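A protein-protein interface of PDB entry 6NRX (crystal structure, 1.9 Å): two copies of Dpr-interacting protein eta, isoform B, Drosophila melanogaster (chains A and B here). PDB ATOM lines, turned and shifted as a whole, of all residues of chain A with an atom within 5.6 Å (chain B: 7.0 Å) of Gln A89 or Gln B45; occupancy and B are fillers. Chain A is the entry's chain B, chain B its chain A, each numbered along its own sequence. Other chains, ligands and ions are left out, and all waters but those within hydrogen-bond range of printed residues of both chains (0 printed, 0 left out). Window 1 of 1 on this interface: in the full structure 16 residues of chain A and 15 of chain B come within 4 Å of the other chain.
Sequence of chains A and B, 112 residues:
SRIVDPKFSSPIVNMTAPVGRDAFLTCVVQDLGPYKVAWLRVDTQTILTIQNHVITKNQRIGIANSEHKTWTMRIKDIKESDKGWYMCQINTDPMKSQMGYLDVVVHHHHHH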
ATOM      1  N   PHE A   8     -33.996  -8.986  20.768  1.00  0.00           N
ATOM      2  CA  PHE A   8     -34.066  -9.630  22.069  1.00  0.00           C
ATOM      3  C   PHE A   8     -35.084  -8.902  22.937  1.00  0.00           C
ATOM      4  O   PHE A   8     -35.055  -7.671  23.043  1.00  0.00           O
ATOM      5  CB  PHE A   8     -32.693  -9.640  22.736  1.00  0.00           C
ATOM      6  CG  PHE A   8     -31.658 -10.417  21.973  1.00  0.00           C
ATOM      7  CD1 PHE A   8     -31.617 -11.800  22.054  1.00  0.00           C
ATOM      8  CD2 PHE A   8     -30.727  -9.770  21.178  1.00  0.00           C
ATOM      9  CE1 PHE A   8     -30.667 -12.520  21.353  1.00  0.00           C
ATOM     10  CE2 PHE A   8     -29.777 -10.483  20.478  1.00  0.00           C
ATOM     11  CZ  PHE A   8     -29.747 -11.860  20.564  1.00  0.00           C
ATOM     12  N   LYS A  36     -32.373 -17.872  12.730  1.00  0.00           N
ATOM     13  CA  LYS A  36     -32.101 -18.988  13.621  1.00  0.00           C
ATOM     14  C   LYS A  36     -31.381 -18.511  14.874  1.00  0.00           C
ATOM     15  O   LYS A  36     -30.604 -17.551  14.841  1.00  0.00           O
ATOM     16  CB  LYS A  36     -31.255 -20.063  12.924  1.00  0.00           C
ATOM     17  CG  LYS A  36     -31.866 -20.587  11.636  1.00  0.00           C
ATOM     18  CD  LYS A  36     -31.134 -21.818  11.126  1.00  0.00           C
ATOM     19  CE  LYS A  36     -31.700 -22.272   9.792  1.00  0.00           C
ATOM     20  NZ  LYS A  36     -33.186 -22.313   9.815  1.00  0.00           N
ATOM     21  N   VAL A  37     -31.643 -19.201  15.980  1.00  0.00           N
ATOM     22  CA  VAL A  37     -31.016 -18.916  17.264  1.00  0.00           C
ATOM     23  C   VAL A  37     -29.984 -19.997  17.549  1.00  0.00           C
ATOM     24  O   VAL A  37     -30.295 -21.194  17.490  1.00  0.00           O
ATOM     25  CB  VAL A  37     -32.062 -18.841  18.388  1.00  0.00           C
ATOM     26  CG1 VAL A  37     -31.382 -18.770  19.751  1.00  0.00           C
ATOM     27  CG2 VAL A  37     -32.978 -17.633  18.169  1.00  0.00           C
ATOM     28  N   ALA A  38     -28.764 -19.579  17.871  1.00  0.00           N
ATOM     29  CA  ALA A  38     -27.671 -20.496  18.164  1.00  0.00           C
ATOM     30  C   ALA A  38     -27.080 -20.188  19.532  1.00  0.00           C
ATOM     31  O   ALA A  38     -26.904 -19.022  19.898  1.00  0.00           O
ATOM     32  CB  ALA A  38     -26.578 -20.412  17.094  1.00  0.00           C
ATOM     33  N   TRP A  39     -26.776 -21.243  20.285  1.00  0.00           N
ATOM     34  CA  TRP A  39     -26.059 -21.126  21.547  1.00  0.00           C
ATOM     35  C   TRP A  39     -24.602 -21.519  21.341  1.00  0.00           C
ATOM     36  O   TRP A  39     -24.302 -22.511  20.670  1.00  0.00           O
ATOM     37  CB  TRP A  39     -26.685 -22.006  22.631  1.00  0.00           C
ATOM     38  CG  TRP A  39     -27.945 -21.451  23.237  1.00  0.00           C
ATOM     39  CD1 TRP A  39     -29.225 -21.770  22.901  1.00  0.00           C
ATOM     40  CD2 TRP A  39     -28.034 -20.493  24.295  1.00  0.00           C
ATOM     41  NE1 TRP A  39     -30.109 -21.064  23.679  1.00  0.00           N
ATOM     42  CE2 TRP A  39     -29.402 -20.271  24.545  1.00  0.00           C
ATOM     43  CE3 TRP A  39     -27.088 -19.796  25.052  1.00  0.00           C
ATOM     44  CZ2 TRP A  39     -29.849 -19.385  25.522  1.00  0.00           C
ATOM     45  CZ3 TRP A  39     -27.535 -18.914  26.022  1.00  0.00           C
ATOM     46  CH2 TRP A  39     -28.900 -18.717  26.248  1.00  0.00           C
ATOM     47  N   LEU A  40     -23.699 -20.727  21.909  1.00  0.00           N
ATOM     48  CA  LEU A  40     -22.271 -20.996  21.843  1.00  0.00           C
ATOM     49  C   LEU A  40     -21.662 -20.775  23.218  1.00  0.00           C
ATOM     50  O   LEU A  40     -22.132 -19.933  23.989  1.00  0.00           O
ATOM     51  CB  LEU A  40     -21.548 -20.094  20.821  1.00  0.00           C
ATOM     52  CG  LEU A  40     -22.024 -20.028  19.367  1.00  0.00           C
ATOM     53  CD1 LEU A  40     -23.197 -19.061  19.216  1.00  0.00           C
ATOM     54  CD2 LEU A  40     -20.867 -19.625  18.454  1.00  0.00           C
ATOM     55  N   ARG A  41     -20.620 -21.541  23.528  1.00  0.00           N
ATOM     56  CA  ARG A  41     -19.820 -21.283  24.718  1.00  0.00           C
ATOM     57  C   ARG A  41     -18.670 -20.361  24.331  1.00  0.00           C
ATOM     58  O   ARG A  41     -17.920 -20.654  23.391  1.00  0.00           O
ATOM     59  CB  ARG A  41     -19.293 -22.576  25.341  1.00  0.00           C
ATOM     60  CG  ARG A  41     -18.452 -22.319  26.582  1.00  0.00           C
ATOM     61  CD  ARG A  41     -18.323 -23.533  27.480  1.00  0.00           C
ATOM     62  NE  ARG A  41     -17.598 -23.196  28.704  1.00  0.00           N
ATOM     63  CZ  ARG A  41     -17.275 -24.069  29.653  1.00  0.00           C
ATOM     64  NH1 ARG A  41     -17.610 -25.345  29.526  1.00  0.00           N
ATOM     65  NH2 ARG A  41     -16.614 -23.664  30.731  1.00  0.00           N
ATOM     66  N   VAL A  42     -18.534 -19.248  25.050  1.00  0.00           N
ATOM     67  CA  VAL A  42     -17.613 -18.201  24.623  1.00  0.00           C
ATOM     68  C   VAL A  42     -16.182 -18.518  25.040  1.00  0.00           C
ATOM     69  O   VAL A  42     -15.241 -18.289  24.272  1.00  0.00           O
ATOM     70  CB  VAL A  42     -18.088 -16.842  25.163  1.00  0.00           C
ATOM     71  CG1 VAL A  42     -17.146 -15.739  24.728  1.00  0.00           C
ATOM     72  CG2 VAL A  42     -19.504 -16.564  24.680  1.00  0.00           C
ATOM     73  N   ASP A  43     -15.989 -19.043  26.253  1.00  0.00           N
ATOM     74  CA  ASP A  43     -14.652 -19.441  26.685  1.00  0.00           C
ATOM     75  C   ASP A  43     -14.051 -20.449  25.715  1.00  0.00           C
ATOM     76  O   ASP A  43     -12.987 -20.218  25.130  1.00  0.00           O
ATOM     77  CB  ASP A  43     -14.704 -20.036  28.095  1.00  0.00           C
ATOM     78  CG  ASP A  43     -15.873 -19.517  28.909  1.00  0.00           C
ATOM     79  OD1 ASP A  43     -17.030 -19.736  28.492  1.00  0.00           O
ATOM     80  OD2 ASP A  43     -15.638 -18.908  29.975  1.00  0.00           O
ATOM     81  N   GLN A  45     -15.095 -21.336  22.801  1.00  0.00           N
ATOM     82  CA  GLN A  45     -15.297 -20.996  21.387  1.00  0.00           C
ATOM     83  C   GLN A  45     -16.059 -22.093  20.644  1.00  0.00           C
ATOM     84  O   GLN A  45     -15.771 -22.394  19.483  1.00  0.00           O
ATOM     85  CB  GLN A  45     -13.963 -20.716  20.688  1.00  0.00           C
ATOM     86  CG  GLN A  45     -13.229 -19.479  21.163  1.00  0.00           C
ATOM     87  CD  GLN A  45     -11.902 -19.300  20.454  1.00  0.00           C
ATOM     88  OE1 GLN A  45     -11.024 -20.161  20.527  1.00  0.00           O
ATOM     89  NE2 GLN A  45     -11.753 -18.184  19.751  1.00  0.00           N
ATOM     90  N   THR A  46     -17.049 -22.685  21.307  1.00  0.00           N
ATOM     91  CA  THR A  46     -17.669 -23.920  20.844  1.00  0.00           C
ATOM     92  C   THR A  46     -19.133 -23.692  20.493  1.00  0.00           C
ATOM     93  O   THR A  46     -19.888 -23.121  21.287  1.00  0.00           O
ATOM     94  CB  THR A  46     -17.552 -25.017  21.908  1.00  0.00           C
ATOM     95  OG1 THR A  46     -16.171 -25.230  22.221  1.00  0.00           O
ATOM     96  CG2 THR A  46     -18.160 -26.320  21.405  1.00  0.00           C
ATOM     97  N   MET A  87     -23.316 -17.594  24.806  1.00  0.00           N
ATOM     98  CA  MET A  87     -23.848 -16.596  23.889  1.00  0.00           C
ATOM     99  C   MET A  87     -25.082 -17.131  23.174  1.00  0.00           C
ATOM    100  O   MET A  87     -25.108 -18.282  22.730  1.00  0.00           O
ATOM    101  CB  MET A  87     -22.788 -16.182  22.860  1.00  0.00           C
ATOM    102  CG  MET A  87     -23.338 -15.409  21.678  1.00  0.00           C
ATOM    103  SD  MET A  87     -22.096 -15.028  20.431  1.00  0.00           S
ATOM    104  CE  MET A  87     -21.055 -13.852  21.296  1.00  0.00           C
ATOM    105  N   CYS A  88     -26.102 -16.282  23.071  1.00  0.00           N
ATOM    106  CA  CYS A  88     -27.286 -16.528  22.253  1.00  0.00           C
ATOM    107  C   CYS A  88     -27.177 -15.637  21.024  1.00  0.00           C
ATOM    108  O   CYS A  88     -27.254 -14.410  21.136  1.00  0.00           O
ATOM    109  CB  CYS A  88     -28.566 -16.236  23.031  1.00  0.00           C
ATOM    110  SG  CYS A  88     -30.064 -16.194  22.021  1.00  0.00           S
ATOM    111  N   GLN A  89     -26.986 -16.247  19.861  1.00  0.00           N
ATOM    112  CA  GLN A  89     -26.613 -15.528  18.651  1.00  0.00           C
ATOM    113  C   GLN A  89     -27.663 -15.734  17.570  1.00  0.00           C
ATOM    114  O   GLN A  89     -28.134 -16.856  17.364  1.00  0.00           O
ATOM    115  CB  GLN A  89     -25.240 -15.998  18.158  1.00  0.00           C
ATOM    116  CG  GLN A  89     -24.933 -15.670  16.712  1.00  0.00           C
ATOM    117  CD  GLN A  89     -23.586 -16.212  16.269  1.00  0.00           C
ATOM    118  OE1 GLN A  89     -23.442 -16.715  15.154  1.00  0.00           O
ATOM    119  NE2 GLN A  89     -22.592 -16.112  17.143  1.00  0.00           N
ATOM    120  N   ILE A  90     -28.014 -14.654  16.872  1.00  0.00           N
ATOM    121  CA  ILE A  90     -28.955 -14.697  15.759  1.00  0.00           C
ATOM    122  C   ILE A  90     -28.189 -14.411  14.475  1.00  0.00           C
ATOM    123  O   ILE A  90     -27.365 -13.491  14.426  1.00  0.00           O
ATOM    124  CB  ILE A  90     -30.099 -13.685  15.956  1.00  0.00           C
ATOM    125  CG1 ILE A  90     -30.688 -13.821  17.364  1.00  0.00           C
ATOM    126  CG2 ILE A  90     -31.174 -13.888  14.899  1.00  0.00           C
ATOM    127  CD1 ILE A  90     -31.739 -12.788  17.680  1.00  0.00           C
ATOM    128  N   ASN A  91     -28.474 -15.186  13.427  1.00  0.00           N
ATOM    129  CA  ASN A  91     -27.740 -15.076  12.165  1.00  0.00           C
ATOM    130  C   ASN A  91     -28.198 -13.911  11.290  1.00  0.00           C
ATOM    131  O   ASN A  91     -28.309 -14.053  10.069  1.00  0.00           O
ATOM    132  CB  ASN A  91     -27.833 -16.398  11.405  1.00  0.00           C
ATOM    133  CG  ASN A  91     -29.254 -16.782  11.062  1.00  0.00           C
ATOM    134  OD1 ASN A  91     -30.207 -16.321  11.688  1.00  0.00           O
ATOM    135  ND2 ASN A  91     -29.404 -17.643  10.061  1.00  0.00           N
ATOM    136  N   MET A  95     -24.287  -9.854  12.620  1.00  0.00           N
ATOM    137  CA  MET A  95     -24.724 -10.763  13.668  1.00  0.00           C
ATOM    138  C   MET A  95     -25.073  -9.992  14.934  1.00  0.00           C
ATOM    139  O   MET A  95     -24.392  -9.035  15.308  1.00  0.00           O
ATOM    140  CB  MET A  95     -23.625 -11.789  13.957  1.00  0.00           C
ATOM    141  CG  MET A  95     -23.967 -12.803  15.030  1.00  0.00           C
ATOM    142  SD  MET A  95     -23.583 -12.266  16.710  1.00  0.00           S
ATOM    143  CE  MET A  95     -21.791 -12.263  16.699  1.00  0.00           C
ATOM    144  N   LYS A  96     -26.144 -10.415  15.597  1.00  0.00           N
ATOM    145  CA  LYS A  96     -26.509  -9.871  16.893  1.00  0.00           C
ATOM    146  C   LYS A  96     -26.614 -11.000  17.910  1.00  0.00           C
ATOM    147  O   LYS A  96     -26.977 -12.134  17.577  1.00  0.00           O
ATOM    148  CB  LYS A  96     -27.817  -9.071  16.826  1.00  0.00           C
ATOM    149  CG  LYS A  96     -29.009  -9.818  16.267  1.00  0.00           C
ATOM    150  CD  LYS A  96     -30.102  -8.836  15.847  1.00  0.00           C
ATOM    151  CE  LYS A  96     -30.362  -7.802  16.932  1.00  0.00           C
ATOM    152  NZ  LYS A  96     -31.534  -6.937  16.610  1.00  0.00           N
ATOM    153  N   SER A  97     -26.281 -10.674  19.155  1.00  0.00           N
ATOM    154  CA  SER A  97     -26.137 -11.675  20.200  1.00  0.00           C
ATOM    155  C   SER A  97     -26.249 -10.995  21.555  1.00  0.00           C
ATOM    156  O   SER A  97     -26.191  -9.768  21.666  1.00  0.00           O
ATOM    157  CB  SER A  97     -24.798 -12.408  20.078  1.00  0.00           C
ATOM    158  OG  SER A  97     -23.717 -11.492  20.146  1.00  0.00           O
ATOM    159  N   GLN A  98     -26.426 -11.817  22.586  1.00  0.00           N
ATOM    160  CA  GLN A  98     -26.237 -11.392  23.962  1.00  0.00           C
ATOM    161  C   GLN A  98     -25.614 -12.546  24.733  1.00  0.00           C
ATOM    162  O   GLN A  98     -25.709 -13.711  24.335  1.00  0.00           O
ATOM    163  CB  GLN A  98     -27.546 -10.930  24.621  1.00  0.00           C
ATOM    164  CG  GLN A  98     -28.765 -11.763  24.290  1.00  0.00           C
ATOM    165  CD  GLN A  98     -30.004 -11.246  24.994  1.00  0.00           C
ATOM    166  OE1 GLN A  98     -30.906 -12.010  25.339  1.00  0.00           O
ATOM    167  NE2 GLN A  98     -30.051  -9.937  25.214  1.00  0.00           N
ATOM    168  N   LEU B  40     -16.347 -20.369  11.265  1.00  0.00           N
ATOM    169  CA  LEU B  40     -16.730 -19.223  12.078  1.00  0.00           C
ATOM    170  C   LEU B  40     -15.754 -18.076  11.855  1.00  0.00           C
ATOM    171  O   LEU B  40     -14.565 -18.291  11.601  1.00  0.00           O
ATOM    172  CB  LEU B  40     -16.768 -19.560  13.582  1.00  0.00           C
ATOM    173  CG  LEU B  40     -17.637 -20.716  14.084  1.00  0.00           C
ATOM    174  CD1 LEU B  40     -16.886 -22.045  14.000  1.00  0.00           C
ATOM    175  CD2 LEU B  40     -18.096 -20.447  15.516  1.00  0.00           C
ATOM    176  N   ARG B  41     -16.271 -16.852  11.953  1.00  0.00           N
ATOM    177  CA  ARG B  41     -15.436 -15.656  11.990  1.00  0.00           C
ATOM    178  C   ARG B  41     -14.993 -15.439  13.432  1.00  0.00           C
ATOM    179  O   ARG B  41     -15.818 -15.163  14.308  1.00  0.00           O
ATOM    180  CB  ARG B  41     -16.201 -14.449  11.450  1.00  0.00           C
ATOM    181  CG  ARG B  41     -15.524 -13.098  11.677  1.00  0.00           C
ATOM    182  CD  ARG B  41     -14.432 -12.815  10.652  1.00  0.00           C
ATOM    183  NE  ARG B  41     -13.678 -11.606  10.979  1.00  0.00           N
ATOM    184  CZ  ARG B  41     -13.888 -10.411  10.433  1.00  0.00           C
ATOM    185  NH1 ARG B  41     -14.832 -10.249   9.516  1.00  0.00           N
ATOM    186  NH2 ARG B  41     -13.147  -9.375  10.802  1.00  0.00           N
ATOM    187  N   VAL B  42     -13.687 -15.563  13.679  1.00  0.00           N
ATOM    188  CA  VAL B  42     -13.183 -15.621  15.051  1.00  0.00           C
ATOM    189  C   VAL B  42     -13.412 -14.310  15.801  1.00  0.00           C
ATOM    190  O   VAL B  42     -13.658 -14.324  17.014  1.00  0.00           O
ATOM    191  CB  VAL B  42     -11.694 -16.019  15.039  1.00  0.00           C
ATOM    192  CG1 VAL B  42     -11.069 -15.809  16.404  1.00  0.00           C
ATOM    193  CG2 VAL B  42     -11.546 -17.469  14.604  1.00  0.00           C
ATOM    194  N   ASP B  43     -13.345 -13.169  15.107  1.00  0.00           N
ATOM    195  CA  ASP B  43     -13.486 -11.867  15.761  1.00  0.00           C
ATOM    196  C   ASP B  43     -14.702 -11.821  16.676  1.00  0.00           C
ATOM    197  O   ASP B  43     -14.614 -11.386  17.829  1.00  0.00           O
ATOM    198  CB  ASP B  43     -13.591 -10.763  14.710  1.00  0.00           C
ATOM    199  CG  ASP B  43     -12.427 -10.761  13.750  1.00  0.00           C
ATOM    200  OD1 ASP B  43     -12.179 -11.803  13.107  1.00  0.00           O
ATOM    201  OD2 ASP B  43     -11.766  -9.710  13.625  1.00  0.00           O
ATOM    202  N   THR B  44     -15.850 -12.272  16.172  1.00  0.00           N
ATOM    203  CA  THR B  44     -17.110 -12.210  16.894  1.00  0.00           C
ATOM    204  C   THR B  44     -17.687 -13.582  17.211  1.00  0.00           C
ATOM    205  O   THR B  44     -18.751 -13.657  17.836  1.00  0.00           O
ATOM    206  CB  THR B  44     -18.141 -11.418  16.081  1.00  0.00           C
ATOM    207  OG1 THR B  44     -18.565 -12.212  14.967  1.00  0.00           O
ATOM    208  CG2 THR B  44     -17.524 -10.138  15.554  1.00  0.00           C
ATOM    209  N   GLN B  45     -17.019 -14.659  16.796  1.00  0.00           N
ATOM    210  CA  GLN B  45     -17.569 -16.013  16.868  1.00  0.00           C
ATOM    211  C   GLN B  45     -18.903 -16.092  16.129  1.00  0.00           C
ATOM    212  O   GLN B  45     -19.833 -16.785  16.548  1.00  0.00           O
ATOM    213  CB  GLN B  45     -17.696 -16.488  18.316  1.00  0.00           C
ATOM    214  CG  GLN B  45     -16.374 -16.429  19.055  1.00  0.00           C
ATOM    215  CD  GLN B  45     -16.440 -17.026  20.440  1.00  0.00           C
ATOM    216  OE1 GLN B  45     -17.035 -18.084  20.649  1.00  0.00           O
ATOM    217  NE2 GLN B  45     -15.828 -16.348  21.400  1.00  0.00           N
ATOM    218  N   THR B  46     -18.991 -15.366  15.014  1.00  0.00           N
ATOM    219  CA  THR B  46     -20.142 -15.453  14.124  1.00  0.00           C
ATOM    220  C   THR B  46     -20.118 -16.790  13.391  1.00  0.00           C
ATOM    221  O   THR B  46     -19.145 -17.108  12.696  1.00  0.00           O
ATOM    222  CB  THR B  46     -20.125 -14.298  13.122  1.00  0.00           C
ATOM    223  OG1 THR B  46     -20.310 -13.057  13.813  1.00  0.00           O
ATOM    224  CG2 THR B  46     -21.233 -14.466  12.106  1.00  0.00           C
ATOM    225  N   ILE B  47     -21.179 -17.578  13.553  1.00  0.00           N
ATOM    226  CA  ILE B  47     -21.300 -18.826  12.809  1.00  0.00           C
ATOM    227  C   ILE B  47     -21.521 -18.495  11.340  1.00  0.00           C
ATOM    228  O   ILE B  47     -22.504 -17.839  10.977  1.00  0.00           O
ATOM    229  CB  ILE B  47     -22.441 -19.690  13.359  1.00  0.00           C
ATOM    230  CG1 ILE B  47     -22.157 -20.086  14.811  1.00  0.00           C
ATOM    231  CG2 ILE B  47     -22.646 -20.923  12.489  1.00  0.00           C
ATOM    232  CD1 ILE B  47     -23.295 -20.832  15.478  1.00  0.00           C
ATOM    233  N   LEU B  48     -20.599 -18.938  10.488  1.00  0.00           N
ATOM    234  CA  LEU B  48     -20.694 -18.689   9.055  1.00  0.00           C
ATOM    235  C   LEU B  48     -21.353 -19.842   8.310  1.00  0.00           C
ATOM    236  O   LEU B  48     -22.334 -19.630   7.587  1.00  0.00           O
ATOM    237  CB  LEU B  48     -19.301 -18.415   8.476  1.00  0.00           C
ATOM    238  CG  LEU B  48     -18.633 -17.140   8.997  1.00  0.00           C
ATOM    239  CD1 LEU B  48     -17.248 -16.951   8.394  1.00  0.00           C
ATOM    240  CD2 LEU B  48     -19.514 -15.934   8.713  1.00  0.00           C
ATOM    241  N   ILE B  55     -24.963 -20.441   7.218  1.00  0.00           N
ATOM    242  CA  ILE B  55     -25.806 -19.989   8.322  1.00  0.00           C
ATOM    243  C   ILE B  55     -25.986 -18.476   8.304  1.00  0.00           C
ATOM    244  O   ILE B  55     -27.094 -17.973   8.511  1.00  0.00           O
ATOM    245  CB  ILE B  55     -25.217 -20.473   9.661  1.00  0.00           C
ATOM    246  CG1 ILE B  55     -25.246 -21.999   9.719  1.00  0.00           C
ATOM    247  CG2 ILE B  55     -26.001 -19.885  10.831  1.00  0.00           C
ATOM    248  CD1 ILE B  55     -26.637 -22.588   9.659  1.00  0.00           C
ATOM    249  N   GLN B  89     -14.042 -25.606  12.572  1.00  0.00           N
ATOM    250  CA  GLN B  89     -14.360 -26.243  13.843  1.00  0.00           C
ATOM    251  C   GLN B  89     -15.129 -27.538  13.616  1.00  0.00           C
ATOM    252  O   GLN B  89     -16.055 -27.580  12.801  1.00  0.00           O
ATOM    253  CB  GLN B  89     -15.170 -25.290  14.731  1.00  0.00           C
ATOM    254  CG  GLN B  89     -15.842 -25.962  15.903  1.00  0.00           C
ATOM    255  CD  GLN B  89     -16.643 -24.998  16.759  1.00  0.00           C
ATOM    256  OE1 GLN B  89     -17.754 -25.312  17.183  1.00  0.00           O
ATOM    257  NE2 GLN B  89     -16.079 -23.824  17.025  1.00  0.00           N
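Hydrophobic or aromatic side chains of chain A within 4 Å of the printed part of chain B: Ala A38, Leu A40, Val A42 and Met A95. Among the printed residues, no Asp or Glu carboxylate lies within 4 Å of a Lys or Arg side-chain nitrogen of the other chain.
O of Ile B55 lies within hydrogen-bond range of ND2 of Asn A91 (2.8 Å). N of Ile B47 sits at hydrogen-bond distance from OE1 of Gln A89. The backbone carbonyl oxygen (O) of Gln A45 sits at hydrogen-bond distance from the side-chain amide nitrogen (NE2) of Gln B89 (2.9 Å). The side-chain amide nitrogen of Gln A89 lies within hydrogen-bond range of the backbone carbonyl oxygen of Gln B45 (2.9 Å).
Ala A38 touches Ile B47. Leu A40 touches Gln B45. Leu A40 touches Ile B47. Arg A41 touches Gln B45. Gln B45 touches Val A42 (NE2 to O, 3.5 Å). OE1 of Gln B45 touches CA of Gln A45, at 3.5 Å. Thr A46 touches Gln B89. CA of Thr B46 touches OE1 of Gln A89, at 3.7 Å. Thr B44 touches Met A95 (O to CE, 3.5 Å). Thr B46 touches Met A95.
Printed residues of chain B within 4 Å of Gln A45: Gln B45 and Gln B89. Printed residues of chain B within 4 Å of Thr A46: Gln B89. Met A87 touches none of the printed residues of chain B. Gln A89 touches just these residues of chain B: Gln B45 (2.9 Å), Thr B46 (3.7 Å) and Ile B47 (2.9 Å). Gln B45 touches just these residues of chain A: Leu A40, Arg A41, Val A42, Gln A45 and Gln A89. The nearest residue of chain B that does not touch Gln A89 is Thr B44 (4.6 Å). The nearest residue of chain A that does not touch Gln B45 is Thr A46 (4.6 Å).
Arg A41 touches Gln B45, but with the chains exchanged Gln A45 does not touch Arg B41 (7.4 Å). Val A42 touches Gln B45, but with the chains exchanged Gln A45 does not touch Val B42 (4.2 Å). Gln A45 touches its own counterpart, Gln B45. Gln A45 touches Gln B89, and with the chains exchanged Gln A89 touches Gln B45. Positions printed for both chains: 40, 41, 42, 43, 45, 46 and 89. Of the 14 pairs that touch across the chains among the printed residues, 5 have their exchanged pair printed and touching as well.
SD of Met A87 lies within hydrogen-bond range of NE2 of Gln A89, at 3.5 Å. The backbone carbonyl oxygen (O) of Thr B46 lies within hydrogen-bond range of the backbone NH (N) of Arg B41, at 3.0 Å. O of Ala A38 is in hydrogen-bond range of N of Gln A89 (2.8 Å). The guanidinium group (NE) of Arg A41 is in salt-bridge range of the side-chain carboxylate (OD1) of Asp A43, at 3.5 Å. The backbone NH (N) of Arg A41 is in hydrogen-bond range of the backbone carbonyl oxygen (O) of Thr A46 (2.8 Å). The side-chain hydroxyl (OG1) of Thr B44 sits close to the backbone NH (N) of Thr B46 (3.2 Å).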
